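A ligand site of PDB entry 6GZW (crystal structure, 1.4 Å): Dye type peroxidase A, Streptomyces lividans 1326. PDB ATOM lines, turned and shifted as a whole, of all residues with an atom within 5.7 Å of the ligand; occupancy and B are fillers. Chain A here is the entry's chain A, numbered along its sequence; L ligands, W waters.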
ATOM      1  N   ASN A 177       5.344  25.789  24.962  1.00  0.00           N
ATOM      2  CA  ASN A 177       6.386  24.776  25.059  1.00  0.00           C
ATOM      3  C   ASN A 177       7.748  25.469  25.304  1.00  0.00           C
ATOM      4  O   ASN A 177       7.822  26.721  25.394  1.00  0.00           O
ATOM      5  CB  ASN A 177       6.365  23.855  23.844  1.00  0.00           C
ATOM      6  CG  ASN A 177       6.680  24.597  22.564  1.00  0.00           C
ATOM      7  OD1 ASN A 177       7.465  25.549  22.600  1.00  0.00           O
ATOM      8  ND2 ASN A 177       6.095  24.178  21.442  1.00  0.00           N
ATOM      9  N   MET A 179      10.272  25.862  23.386  1.00  0.00           N
ATOM     10  CA  MET A 179      10.669  26.774  22.295  1.00  0.00           C
ATOM     11  C   MET A 179       9.957  28.128  22.365  1.00  0.00           C
ATOM     12  O   MET A 179      10.218  29.026  21.516  1.00  0.00           O
ATOM     13  CB  MET A 179      10.423  26.072  20.941  1.00  0.00           C
ATOM     14  CG  MET A 179      11.539  25.085  20.583  1.00  0.00           C
ATOM     15  SD  MET A 179      11.092  24.127  19.135  1.00  0.00           S
ATOM     16  CE  MET A 179      12.718  23.687  18.571  1.00  0.00           C
ATOM     17  N   GLN A 181       6.773  28.661  21.890  1.00  0.00           N
ATOM     18  CA  GLN A 181       5.616  28.683  21.009  1.00  0.00           C
ATOM     19  C   GLN A 181       4.292  28.477  21.745  1.00  0.00           C
ATOM     20  O   GLN A 181       4.217  27.692  22.686  1.00  0.00           O
ATOM     21  CB  GLN A 181       5.755  27.592  19.936  1.00  0.00           C
ATOM     22  CG  GLN A 181       6.959  27.788  19.023  1.00  0.00           C
ATOM     23  CD  GLN A 181       7.674  26.514  18.581  1.00  0.00           C
ATOM     24  OE1 GLN A 181       7.329  25.396  19.004  1.00  0.00           O
ATOM     25  NE2 GLN A 181       8.719  26.676  17.757  1.00  0.00           N
ATOM     26  N   VAL A 182       3.228  29.113  21.265  1.00  0.00           N
ATOM     27  CA  VAL A 182       1.871  28.698  21.607  1.00  0.00           C
ATOM     28  C   VAL A 182       1.705  27.282  21.051  1.00  0.00           C
ATOM     29  O   VAL A 182       1.963  27.041  19.874  1.00  0.00           O
ATOM     30  CB  VAL A 182       0.819  29.658  21.016  1.00  0.00           C
ATOM     31  CG1 VAL A 182      -0.599  29.167  21.300  1.00  0.00           C
ATOM     32  CG2 VAL A 182       1.000  31.062  21.567  1.00  0.00           C
ATOM     33  N   ASP A 183       1.283  26.345  21.893  1.00  0.00           N
ATOM     34  CA  ASP A 183       1.212  24.937  21.492  1.00  0.00           C
ATOM     35  C   ASP A 183      -0.100  24.317  22.005  1.00  0.00           C
ATOM     36  O   ASP A 183      -0.325  24.177  23.221  1.00  0.00           O
ATOM     37  CB  ASP A 183       2.439  24.183  22.047  1.00  0.00           C
ATOM     38  CG  ASP A 183       2.661  22.828  21.402  1.00  0.00           C
ATOM     39  OD1 ASP A 183       1.682  22.207  20.897  1.00  0.00           O
ATOM     40  OD2 ASP A 183       3.826  22.352  21.347  1.00  0.00           O
ATOM     41  N   GLY A 184      -0.962  23.940  21.064  1.00  0.00           N
ATOM     42  CA  GLY A 184      -2.243  23.322  21.380  1.00  0.00           C
ATOM     43  C   GLY A 184      -3.439  23.947  20.695  1.00  0.00           C
ATOM     44  O   GLY A 184      -4.544  23.411  20.794  1.00  0.00           O
ATOM     45  N   THR A 185      -3.264  25.052  19.975  1.00  0.00           N
ATOM     46  CA  THR A 185      -4.402  25.767  19.383  1.00  0.00           C
ATOM     47  C   THR A 185      -5.317  24.862  18.543  1.00  0.00           C
ATOM     48  O   THR A 185      -6.532  24.881  18.728  1.00  0.00           O
ATOM     49  CB  THR A 185      -3.860  26.897  18.497  1.00  0.00           C
ATOM     50  OG1 THR A 185      -3.043  27.756  19.293  1.00  0.00           O
ATOM     51  CG2 THR A 185      -4.970  27.660  17.838  1.00  0.00           C
ATOM     52  N   ARG A 186      -4.721  24.084  17.639  1.00  0.00           N
ATOM     53  CA  ARG A 186      -5.490  23.255  16.692  1.00  0.00           C
ATOM     54  C   ARG A 186      -5.602  21.800  17.145  1.00  0.00           C
ATOM     55  O   ARG A 186      -5.484  20.857  16.360  1.00  0.00           O
ATOM     56  CB  ARG A 186      -4.932  23.409  15.282  1.00  0.00           C
ATOM     57  CG  ARG A 186      -5.198  24.809  14.685  1.00  0.00           C
ATOM     58  CD  ARG A 186      -6.256  24.806  13.557  1.00  0.00           C
ATOM     59  NE  ARG A 186      -5.839  23.838  12.538  1.00  0.00           N
ATOM     60  CZ  ARG A 186      -6.597  23.425  11.522  1.00  0.00           C
ATOM     61  NH1 ARG A 186      -7.818  23.922  11.361  1.00  0.00           N
ATOM     62  NH2 ARG A 186      -6.140  22.494  10.702  1.00  0.00           N
ATOM     63  N   ASN A 187      -5.848  21.621  18.425  1.00  0.00           N
ATOM     64  CA  ASN A 187      -6.020  20.292  18.976  1.00  0.00           C
ATOM     65  C   ASN A 187      -7.486  19.962  18.831  1.00  0.00           C
ATOM     66  O   ASN A 187      -8.327  20.729  19.317  1.00  0.00           O
ATOM     67  CB  ASN A 187      -5.618  20.297  20.456  1.00  0.00           C
ATOM     68  CG  ASN A 187      -5.581  18.913  21.062  1.00  0.00           C
ATOM     69  OD1 ASN A 187      -5.173  17.943  20.405  1.00  0.00           O
ATOM     70  ND2 ASN A 187      -5.962  18.818  22.342  1.00  0.00           N
ATOM     71  N   ARG A 224       6.641  10.265  22.054  1.00  0.00           N
ATOM     72  CA  ARG A 224       7.989  10.575  21.533  1.00  0.00           C
ATOM     73  C   ARG A 224       8.678  11.516  22.489  1.00  0.00           C
ATOM     74  O   ARG A 224       8.122  12.568  22.837  1.00  0.00           O
ATOM     75  CB  ARG A 224       7.921  11.241  20.145  1.00  0.00           C
ATOM     76  CG  ARG A 224       7.099  10.450  19.121  1.00  0.00           C
ATOM     77  CD  ARG A 224       7.791   9.181  18.645  1.00  0.00           C
ATOM     78  NE  ARG A 224       8.831   9.488  17.669  1.00  0.00           N
ATOM     79  CZ  ARG A 224       9.333   8.627  16.774  1.00  0.00           C
ATOM     80  NH1 ARG A 224       8.948   7.344  16.762  1.00  0.00           N
ATOM     81  NH2 ARG A 224      10.253   9.053  15.898  1.00  0.00           N
ATOM     82  N   ILE A 226      11.118  14.090  22.515  1.00  0.00           N
ATOM     83  CA  ILE A 226      11.725  14.904  21.468  1.00  0.00           C
ATOM     84  C   ILE A 226      12.554  15.995  22.144  1.00  0.00           C
ATOM     85  O   ILE A 226      12.013  16.908  22.761  1.00  0.00           O
ATOM     86  CB  ILE A 226      10.661  15.550  20.554  1.00  0.00           C
ATOM     87  CG1 ILE A 226       9.693  14.481  20.033  1.00  0.00           C
ATOM     88  CG2 ILE A 226      11.343  16.261  19.402  1.00  0.00           C
ATOM     89  CD1 ILE A 226       8.580  15.056  19.185  1.00  0.00           C
ATOM     90  N   ARG A 227      13.879  15.881  22.024  1.00  0.00           N
ATOM     91  CA  ARG A 227      14.753  16.873  22.575  1.00  0.00           C
ATOM     92  C   ARG A 227      14.689  18.103  21.714  1.00  0.00           C
ATOM     93  O   ARG A 227      14.637  18.019  20.490  1.00  0.00           O
ATOM     94  CB  ARG A 227      16.201  16.377  22.652  1.00  0.00           C
ATOM     95  CG  ARG A 227      17.165  17.393  23.240  1.00  0.00           C
ATOM     96  CD  ARG A 227      18.407  16.747  23.808  1.00  0.00           C
ATOM     97  NE  ARG A 227      19.260  16.151  22.781  1.00  0.00           N
ATOM     98  CZ  ARG A 227      20.222  16.797  22.121  1.00  0.00           C
ATOM     99  NH1 ARG A 227      20.441  18.093  22.311  1.00  0.00           N
ATOM    100  NH2 ARG A 227      20.954  16.134  21.244  1.00  0.00           N
ATOM    101  N   MET A 228      14.618  19.255  22.344  1.00  0.00           N
ATOM    102  CA  MET A 228      14.706  20.493  21.603  1.00  0.00           C
ATOM    103  C   MET A 228      16.148  20.960  21.570  1.00  0.00           C
ATOM    104  O   MET A 228      16.775  21.059  22.584  1.00  0.00           O
ATOM    105  CB  MET A 228      13.820  21.565  22.220  1.00  0.00           C
ATOM    106  CG  MET A 228      12.332  21.297  22.060  1.00  0.00           C
ATOM    107  SD  MET A 228      11.355  22.304  23.173  1.00  0.00           S
ATOM    108  CE  MET A 228       9.779  22.177  22.352  1.00  0.00           C
ATOM    109  N   ILE A 245       7.521  27.615  12.128  1.00  0.00           N
ATOM    110  CA  ILE A 245       6.189  27.117  12.538  1.00  0.00           C
ATOM    111  C   ILE A 245       5.076  27.580  11.584  1.00  0.00           C
ATOM    112  O   ILE A 245       4.171  26.813  11.300  1.00  0.00           O
ATOM    113  CB  ILE A 245       5.844  27.570  13.974  1.00  0.00           C
ATOM    114  CG1 ILE A 245       6.845  26.986  14.979  1.00  0.00           C
ATOM    115  CG2 ILE A 245       4.410  27.196  14.348  1.00  0.00           C
ATOM    116  CD1 ILE A 245       6.897  25.468  15.017  1.00  0.00           C
ATOM    117  N   ARG A 247       3.318  30.339  12.503  1.00  0.00           N
ATOM    118  CA  ARG A 247       2.480  31.046  13.435  1.00  0.00           C
ATOM    119  C   ARG A 247       3.353  31.952  14.303  1.00  0.00           C
ATOM    120  O   ARG A 247       4.522  31.669  14.535  1.00  0.00           O
ATOM    121  CB  ARG A 247       1.726  30.076  14.341  1.00  0.00           C
ATOM    122  CG  ARG A 247       0.604  29.343  13.649  1.00  0.00           C
ATOM    123  CD  ARG A 247      -0.043  28.259  14.480  1.00  0.00           C
ATOM    124  NE  ARG A 247      -1.169  27.618  13.787  1.00  0.00           N
ATOM    125  CZ  ARG A 247      -2.390  28.141  13.669  1.00  0.00           C
ATOM    126  NH1 ARG A 247      -2.693  29.319  14.179  1.00  0.00           N
ATOM    127  NH2 ARG A 247      -3.363  27.438  13.044  1.00  0.00           N
ATOM    128  N   HIS A 285       5.915  24.043   9.888  1.00  0.00           N
ATOM    129  CA  HIS A 285       5.328  22.938  10.673  1.00  0.00           C
ATOM    130  C   HIS A 285       3.796  22.979  10.774  1.00  0.00           C
ATOM    131  O   HIS A 285       3.122  21.973  10.584  1.00  0.00           O
ATOM    132  CB  HIS A 285       5.943  23.005  12.073  1.00  0.00           C
ATOM    133  CG  HIS A 285       5.510  21.902  12.967  1.00  0.00           C
ATOM    134  ND1 HIS A 285       6.047  20.634  12.892  1.00  0.00           N
ATOM    135  CD2 HIS A 285       4.581  21.886  13.944  1.00  0.00           C
ATOM    136  CE1 HIS A 285       5.468  19.876  13.817  1.00  0.00           C
ATOM    137  NE2 HIS A 285       4.570  20.612  14.470  1.00  0.00           N
ATOM    138  N   ALA A 286       3.266  24.150  11.076  1.00  0.00           N
ATOM    139  CA  ALA A 286       1.816  24.328  11.226  1.00  0.00           C
ATOM    140  C   ALA A 286       1.051  24.391   9.897  1.00  0.00           C
ATOM    141  O   ALA A 286      -0.199  24.439   9.900  1.00  0.00           O
ATOM    142  CB  ALA A 286       1.471  25.513  12.133  1.00  0.00           C
ATOM    143  N   THR A 289       1.589  19.833   8.939  1.00  0.00           N
ATOM    144  CA  THR A 289       0.969  18.878   9.875  1.00  0.00           C
ATOM    145  C   THR A 289      -0.578  18.857   9.832  1.00  0.00           C
ATOM    146  O   THR A 289      -1.202  17.973  10.432  1.00  0.00           O
ATOM    147  CB  THR A 289       1.362  19.239  11.329  1.00  0.00           C
ATOM    148  OG1 THR A 289       1.035  20.613  11.529  1.00  0.00           O
ATOM    149  CG2 THR A 289       2.820  18.996  11.579  1.00  0.00           C
ATOM    150  N   ARG A 290      -1.220  19.782   9.102  1.00  0.00           N
ATOM    151  CA  ARG A 290      -2.688  19.861   9.110  1.00  0.00           C
ATOM    152  C   ARG A 290      -3.340  18.596   8.527  1.00  0.00           C
ATOM    153  O   ARG A 290      -2.822  17.995   7.564  1.00  0.00           O
ATOM    154  CB  ARG A 290      -3.168  21.070   8.316  1.00  0.00           C
ATOM    155  CG  ARG A 290      -2.775  22.456   8.853  1.00  0.00           C
ATOM    156  CD  ARG A 290      -2.941  23.537   7.778  1.00  0.00           C
ATOM    157  NE  ARG A 290      -4.339  23.655   7.397  1.00  0.00           N
ATOM    158  CZ  ARG A 290      -5.220  24.523   7.909  1.00  0.00           C
ATOM    159  NH1 ARG A 290      -4.882  25.387   8.873  1.00  0.00           N
ATOM    160  NH2 ARG A 290      -6.495  24.507   7.469  1.00  0.00           N
ATOM    161  N   PRO A 291      -4.489  18.186   9.107  1.00  0.00           N
ATOM    162  CA  PRO A 291      -5.208  17.071   8.483  1.00  0.00           C
ATOM    163  C   PRO A 291      -5.512  17.312   6.999  1.00  0.00           C
ATOM    164  O   PRO A 291      -5.372  16.379   6.214  1.00  0.00           O
ATOM    165  CB  PRO A 291      -6.475  16.932   9.356  1.00  0.00           C
ATOM    166  CG  PRO A 291      -6.075  17.474  10.715  1.00  0.00           C
ATOM    167  CD  PRO A 291      -5.082  18.571  10.410  1.00  0.00           C
ATOM    168  N   MET A 299      -4.780  13.773  14.919  1.00  0.00           N
ATOM    169  CA  MET A 299      -4.470  13.230  16.235  1.00  0.00           C
ATOM    170  C   MET A 299      -4.790  14.279  17.287  1.00  0.00           C
ATOM    171  O   MET A 299      -4.733  15.460  17.006  1.00  0.00           O
ATOM    172  CB  MET A 299      -2.984  12.831  16.304  1.00  0.00           C
ATOM    173  CG  MET A 299      -2.011  14.012  16.287  1.00  0.00           C
ATOM    174  SD  MET A 299      -0.396  13.609  15.618  1.00  0.00           S
ATOM    175  CE  MET A 299      -0.887  13.550  13.895  1.00  0.00           C
ATOM    176  N   ARG A 301      -3.190  15.919  20.544  1.00  0.00           N
ATOM    177  CA  ARG A 301      -1.869  16.136  21.155  1.00  0.00           C
ATOM    178  C   ARG A 301      -2.076  16.591  22.587  1.00  0.00           C
ATOM    179  O   ARG A 301      -2.865  17.491  22.853  1.00  0.00           O
ATOM    180  CB  ARG A 301      -1.107  17.190  20.363  1.00  0.00           C
ATOM    181  CG  ARG A 301      -0.708  16.699  18.970  1.00  0.00           C
ATOM    182  CD  ARG A 301      -0.096  17.787  18.110  1.00  0.00           C
ATOM    183  NE  ARG A 301      -1.111  18.807  17.860  1.00  0.00           N
ATOM    184  CZ  ARG A 301      -1.021  20.115  18.115  1.00  0.00           C
ATOM    185  NH1 ARG A 301       0.065  20.669  18.653  1.00  0.00           N
ATOM    186  NH2 ARG A 301      -2.058  20.885  17.793  1.00  0.00           N
ATOM    187  N   LEU A 320      10.187  18.097  24.661  1.00  0.00           N
ATOM    188  CA  LEU A 320       8.748  17.801  24.753  1.00  0.00           C
ATOM    189  C   LEU A 320       8.528  16.321  24.817  1.00  0.00           C
ATOM    190  O   LEU A 320       9.097  15.566  24.001  1.00  0.00           O
ATOM    191  CB  LEU A 320       8.066  18.335  23.485  1.00  0.00           C
ATOM    192  CG  LEU A 320       6.528  18.392  23.501  1.00  0.00           C
ATOM    193  CD1 LEU A 320       6.020  19.479  24.414  1.00  0.00           C
ATOM    194  CD2 LEU A 320       6.041  18.618  22.073  1.00  0.00           C
ATOM    195  N   PHE A 322       6.120  14.360  23.699  1.00  0.00           N
ATOM    196  CA  PHE A 322       5.031  14.420  22.734  1.00  0.00           C
ATOM    197  C   PHE A 322       4.183  13.170  22.971  1.00  0.00           C
ATOM    198  O   PHE A 322       4.698  12.069  22.966  1.00  0.00           O
ATOM    199  CB  PHE A 322       5.636  14.444  21.340  1.00  0.00           C
ATOM    200  CG  PHE A 322       4.632  14.560  20.229  1.00  0.00           C
ATOM    201  CD1 PHE A 322       4.170  15.805  19.817  1.00  0.00           C
ATOM    202  CD2 PHE A 322       4.146  13.429  19.605  1.00  0.00           C
ATOM    203  CE1 PHE A 322       3.240  15.929  18.772  1.00  0.00           C
ATOM    204  CE2 PHE A 322       3.228  13.547  18.566  1.00  0.00           C
ATOM    205  CZ  PHE A 322       2.775  14.800  18.161  1.00  0.00           C
ATOM    206  N   PHE A 333      -0.347   9.839  13.577  1.00  0.00           N
ATOM    207  CA  PHE A 333       1.093  10.052  13.736  1.00  0.00           C
ATOM    208  C   PHE A 333       1.946   9.609  12.553  1.00  0.00           C
ATOM    209  O   PHE A 333       2.802  10.373  12.098  1.00  0.00           O
ATOM    210  CB  PHE A 333       1.611   9.370  15.012  1.00  0.00           C
ATOM    211  CG  PHE A 333       3.099   9.509  15.207  1.00  0.00           C
ATOM    212  CD1 PHE A 333       3.609  10.666  15.766  1.00  0.00           C
ATOM    213  CD2 PHE A 333       3.979   8.531  14.785  1.00  0.00           C
ATOM    214  CE1 PHE A 333       4.988  10.822  15.931  1.00  0.00           C
ATOM    215  CE2 PHE A 333       5.356   8.688  14.907  1.00  0.00           C
ATOM    216  CZ  PHE A 333       5.859   9.836  15.503  1.00  0.00           C
ATOM    217  N   VAL A 336       1.906  11.699   9.120  1.00  0.00           N
ATOM    218  CA  VAL A 336       2.345  13.054   9.390  1.00  0.00           C
ATOM    219  C   VAL A 336       3.850  13.022   9.647  1.00  0.00           C
ATOM    220  O   VAL A 336       4.590  13.813   9.055  1.00  0.00           O
ATOM    221  CB  VAL A 336       1.560  13.705  10.539  1.00  0.00           C
ATOM    222  CG1 VAL A 336       2.121  15.079  10.865  1.00  0.00           C
ATOM    223  CG2 VAL A 336       0.073  13.797  10.196  1.00  0.00           C
ATOM    224  N   GLN A 337       4.324  12.138  10.523  1.00  0.00           N
ATOM    225  CA  GLN A 337       5.768  12.044  10.764  1.00  0.00           C
ATOM    226  C   GLN A 337       6.579  11.675   9.521  1.00  0.00           C
ATOM    227  O   GLN A 337       7.685  12.185   9.346  1.00  0.00           O
ATOM    228  CB  GLN A 337       6.092  11.120  11.965  1.00  0.00           C
ATOM    229  CG  GLN A 337       7.553  11.094  12.414  1.00  0.00           C
ATOM    230  CD  GLN A 337       8.128  12.462  12.788  1.00  0.00           C
ATOM    231  OE1 GLN A 337       7.391  13.386  13.129  1.00  0.00           O
ATOM    232  NE2 GLN A 337       9.452  12.587  12.738  1.00  0.00           N
ATOM    233  N   LEU A 340       6.946  14.942   8.036  1.00  0.00           N
ATOM    234  CA  LEU A 340       7.833  15.860   8.778  1.00  0.00           C
ATOM    235  C   LEU A 340       9.314  15.493   8.697  1.00  0.00           C
ATOM    236  O   LEU A 340      10.200  16.385   8.735  1.00  0.00           O
ATOM    237  CB  LEU A 340       7.444  15.916  10.265  1.00  0.00           C
ATOM    238  CG  LEU A 340       6.009  16.268  10.632  1.00  0.00           C
ATOM    239  CD1 LEU A 340       5.919  16.493  12.129  1.00  0.00           C
ATOM    240  CD2 LEU A 340       5.484  17.464   9.857  1.00  0.00           C
ATOM    241  N   LEU A 346      10.963  22.456  11.093  1.00  0.00           N
ATOM    242  CA  LEU A 346      11.251  22.235  12.529  1.00  0.00           C
ATOM    243  C   LEU A 346      12.244  21.112  12.769  1.00  0.00           C
ATOM    244  O   LEU A 346      12.906  21.093  13.815  1.00  0.00           O
ATOM    245  CB  LEU A 346       9.961  21.947  13.285  1.00  0.00           C
ATOM    246  CG  LEU A 346      10.042  21.693  14.788  1.00  0.00           C
ATOM    247  CD1 LEU A 346      10.550  22.932  15.476  1.00  0.00           C
ATOM    248  CD2 LEU A 346       8.709  21.220  15.350  1.00  0.00           C
ATOM    249  N   ILE A 350      15.048  19.765  16.377  1.00  0.00           N
ATOM    250  CA  ILE A 350      14.585  18.757  17.302  1.00  0.00           C
ATOM    251  C   ILE A 350      15.276  17.390  17.068  1.00  0.00           C
ATOM    252  O   ILE A 350      15.846  17.125  15.999  1.00  0.00           O
ATOM    253  CB  ILE A 350      13.061  18.610  17.275  1.00  0.00           C
ATOM    254  CG1 ILE A 350      12.585  18.124  15.881  1.00  0.00           C
ATOM    255  CG2 ILE A 350      12.361  19.893  17.699  1.00  0.00           C
ATOM    256  CD1 ILE A 350      11.126  17.736  15.843  1.00  0.00           C
ATOM    257  N   HIS A 352      14.293  13.255  17.901  1.00  0.00           N
ATOM    258  CA  HIS A 352      13.457  12.233  18.507  1.00  0.00           C
ATOM    259  C   HIS A 352      14.376  11.170  19.156  1.00  0.00           C
ATOM    260  O   HIS A 352      15.164  10.466  18.473  1.00  0.00           O
ATOM    261  CB  HIS A 352      12.576  11.549  17.484  1.00  0.00           C
ATOM    262  CG  HIS A 352      11.471  12.410  16.939  1.00  0.00           C
ATOM    263  ND1 HIS A 352      10.139  12.095  17.096  1.00  0.00           N
ATOM    264  CD2 HIS A 352      11.506  13.542  16.191  1.00  0.00           C
ATOM    265  CE1 HIS A 352       9.394  13.006  16.485  1.00  0.00           C
ATOM    266  NE2 HIS A 352      10.196  13.888  15.919  1.00  0.00           N
HETATM  267  C1  LIG L   1       0.912  22.078  15.559  1.00  0.00           C
HETATM  268  C2  LIG L   1       5.161  22.610  17.806  1.00  0.00           C
HETATM  269  C3  LIG L   1       6.098  17.909  17.020  1.00  0.00           C
HETATM  270  C4  LIG L   1       1.869  17.394  14.787  1.00  0.00           C
HETATM  271  C5  LIG L   1       1.976  22.627  16.226  1.00  0.00           C
HETATM  272  C6  LIG L   1       2.080  24.006  16.570  1.00  0.00           C
HETATM  273  C7  LIG L   1       3.282  24.137  17.201  1.00  0.00           C
HETATM  274  C8  LIG L   1       3.908  22.856  17.241  1.00  0.00           C
HETATM  275  C9  LIG L   1       3.879  25.396  17.797  1.00  0.00           C
HETATM  276  C10 LIG L   1       1.087  25.115  16.287  1.00  0.00           C
HETATM  277  C11 LIG L   1       0.015  25.379  17.339  1.00  0.00           C
HETATM  278  C12 LIG L   1      -0.947  24.254  17.436  1.00  0.00           C
HETATM  279  O1  LIG L   1      -1.938  24.137  16.651  1.00  0.00           O
HETATM  280  O2  LIG L   1      -0.787  23.355  18.314  1.00  0.00           O
HETATM  281  C13 LIG L   1       5.788  21.351  17.801  1.00  0.00           C
HETATM  282  C14 LIG L   1       7.036  21.068  18.434  1.00  0.00           C
HETATM  283  C15 LIG L   1       7.338  19.762  18.232  1.00  0.00           C
HETATM  284  C16 LIG L   1       6.182  19.212  17.440  1.00  0.00           C
HETATM  285  C17 LIG L   1       7.889  22.068  19.157  1.00  0.00           C
HETATM  286  C18 LIG L   1       8.456  18.946  18.748  1.00  0.00           C
HETATM  287  C19 LIG L   1       9.127  19.219  19.847  1.00  0.00           C
HETATM  288  C20 LIG L   1       5.065  17.358  16.297  1.00  0.00           C
HETATM  289  C21 LIG L   1       5.006  16.009  15.868  1.00  0.00           C
HETATM  290  C22 LIG L   1       3.791  15.869  15.221  1.00  0.00           C
HETATM  291  C23 LIG L   1       3.112  17.134  15.290  1.00  0.00           C
HETATM  292  C24 LIG L   1       6.041  14.949  16.045  1.00  0.00           C
HETATM  293  C25 LIG L   1       3.221  14.694  14.514  1.00  0.00           C
HETATM  294  C26 LIG L   1       3.894  13.652  13.986  1.00  0.00           C
HETATM  295  C27 LIG L   1       1.267  18.660  14.910  1.00  0.00           C
HETATM  296  C28 LIG L   1      -0.101  18.869  14.406  1.00  0.00           C
HETATM  297  C29 LIG L   1      -0.376  20.171  14.619  1.00  0.00           C
HETATM  298  C30 LIG L   1       0.851  20.740  15.238  1.00  0.00           C
HETATM  299  C31 LIG L   1      -1.039  17.820  13.818  1.00  0.00           C
HETATM  300  C32 LIG L   1      -1.682  20.869  14.261  1.00  0.00           C
HETATM  301  C33 LIG L   1      -1.726  21.311  12.792  1.00  0.00           C
HETATM  302  C34 LIG L   1      -3.048  21.927  12.465  1.00  0.00           C
HETATM  303  O3  LIG L   1      -3.201  23.183  12.530  1.00  0.00           O
HETATM  304  O4  LIG L   1      -3.994  21.184  12.165  1.00  0.00           O
HETATM  305  N1  LIG L   1       3.133  21.949  16.548  1.00  0.00           N
HETATM  306  N2  LIG L   1       5.341  20.231  17.215  1.00  0.00           N
HETATM  307  N3  LIG L   1       3.960  18.037  15.898  1.00  0.00           N
HETATM  308  N4  LIG L   1       1.842  19.807  15.312  1.00  0.00           N
HETATM  309 FE1  LIG L   1       3.537  20.025  16.200  1.00  0.00          FE
HETATM  310  O   HOH W   1       1.734  28.399  17.603  1.00  0.00           O
HETATM  311  O   HOH W   2      -5.259  19.430  13.914  1.00  0.00           O
HETATM  312  O   HOH W   3      -2.833  16.078  11.567  1.00  0.00           O
HETATM  313  O   HOH W   4      -4.289  16.617  13.892  1.00  0.00           O
HETATM  314  O   HOH W   5       4.055  20.165  20.091  1.00  0.00           O
HETATM  315  O   HOH W   6      -1.522  24.830  14.006  1.00  0.00           O
HETATM  316  O   HOH W   7       2.746  19.494  17.935  1.00  0.00           O
HETATM  317  O   HOH W   8      -2.664  25.313  10.872  1.00  0.00           O
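Asn 177 touches the ligand.
Met 179 touches the ligand.
Gln 181 touches the ligand (OE1 to C17, 3.4 Å).
O of Val 182 touches C9 of the ligand, 3.3 Å away.
Asp 183 touches the ligand (OD1 to O2, 3.8 Å).
CG2 of Ile 226 touches C19 of the ligand (3.7 Å).
CE of Met 228 touches C17 of the ligand, at 3.7 Å.
CG2 of Ile 245 touches C9 of the ligand (3.9 Å).
CD of Arg 247 touches C10 of the ligand, at 3.8 Å.
Thr 289 touches the ligand (OG1 to C33, 3.1 Å).
Arg 290 touches the ligand (CA to O4, 3.6 Å).
Pro 291 touches the ligand.
Met 299 touches the ligand.
Leu 320 touches the ligand (CD2 to C19, 3.9 Å).
Phe 322 touches the ligand (CZ to C22, 3.3 Å).
Phe 333 touches the ligand (CD1 to C26, 3.5 Å).
Val 336 touches the ligand.
Gln 337 touches the ligand.
Leu 340 touches the ligand.
Leu 346 touches the ligand (CD2 to C15, 3.5 Å).
CG2 of Ile 350 touches C19 of the ligand, at 3.9 Å.
His 352 touches the ligand (CE1 to C24, 3.9 Å).
Hydrophobic or aromatic side chains that line the ligand: Met 179, Ile 226, Met 228, Ile 245, His 285, Pro 291, Met 299, Leu 320, Phe 322, Phe 333, Val 336, Leu 340, Leu 346, Ile 350 and His 352.
27 residues have an atom within 4 Å of the ligand: Asn 177, Met 179, Gln 181, Val 182, Asp 183, Gly 184, Thr 185, Arg 186, Ile 226, Met 228, Ile 245, Arg 247, His 285, Thr 289, Arg 290, Pro 291, Met 299, Arg 301, Leu 320, Phe 322, Phe 333, Val 336, Gln 337, Leu 340, Leu 346, Ile 350 and His 352.
Along chain A the residues within 4 Å of the ligand span positions 177 to 352.
The nearest printed residue that does not touch the ligand is Ala 286 (4.2 Å).
Water W8 lies within hydrogen-bond range of O3 of the ligand (2.8 Å), O of Ala 286 (2.8 Å), NH1 of Arg 290 (3.0 Å) and NH2 of Arg 247 (3.1 Å).
Water W6 lies within hydrogen-bond range of an oxygen (O1) of the ligand (2.8 Å) and the guanidinium group (NE) of Arg 247 (2.8 Å).
Water W2 lies within hydrogen-bond range of O4 of the ligand (2.8 Å) and O of Arg 186 (2.8 Å).
The backbone carbonyl oxygen (O) of His 285 lies within hydrogen-bond range of the side-chain hydroxyl (OG1) of Thr 289 (2.7 Å).
The backbone carbonyl oxygen (O) of Phe 322 sits at hydrogen-bond distance from the backbone NH (N) of Arg 224 (2.8 Å).
The side-chain amide oxygen (OE1) of Gln 181 is in hydrogen-bond range of the side-chain amide nitrogen (ND2) of Asn 177, 3.0 Å away.
The side-chain amide nitrogen (NE2) of Gln 181 sits close to the side-chain sulfur (SD) of Met 179 (3.7 Å).
The side-chain carboxylate (OD2) of Asp 183 sits at hydrogen-bond distance from the side-chain amide nitrogen (ND2) of Asn 177 (2.9 Å).
The side-chain amide oxygen (OD1) of Asn 177 sits at hydrogen-bond distance from the backbone NH (N) of Met 179, 2.9 Å away.
SD of Met 228 lies within hydrogen-bond range of N of Met 179, 3.7 Å away.
ND1 of His 352 is in hydrogen-bond range of NE of Arg 224 (3.0 Å).
NE2 of His 285 binds FE1 of the ligand, at 2.1 Å.
The backbone NH of Arg 186 sits at hydrogen-bond distance from an oxygen (O1) of the ligand (3.0 Å).
An oxygen (O3) of the ligand is in salt-bridge range of the guanidinium group (NE) of Arg 186 (2.7 Å).
The backbone NH of Gly 184 lies within hydrogen-bond range of an oxygen (O2) of the ligand (2.8 Å).
An oxygen (O2) of the ligand lies within salt-bridge range of the guanidinium group (NH2) of Arg 301 (2.8 Å).
O2 of the ligand sits at hydrogen-bond distance from N of Thr 185 (3.4 Å).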
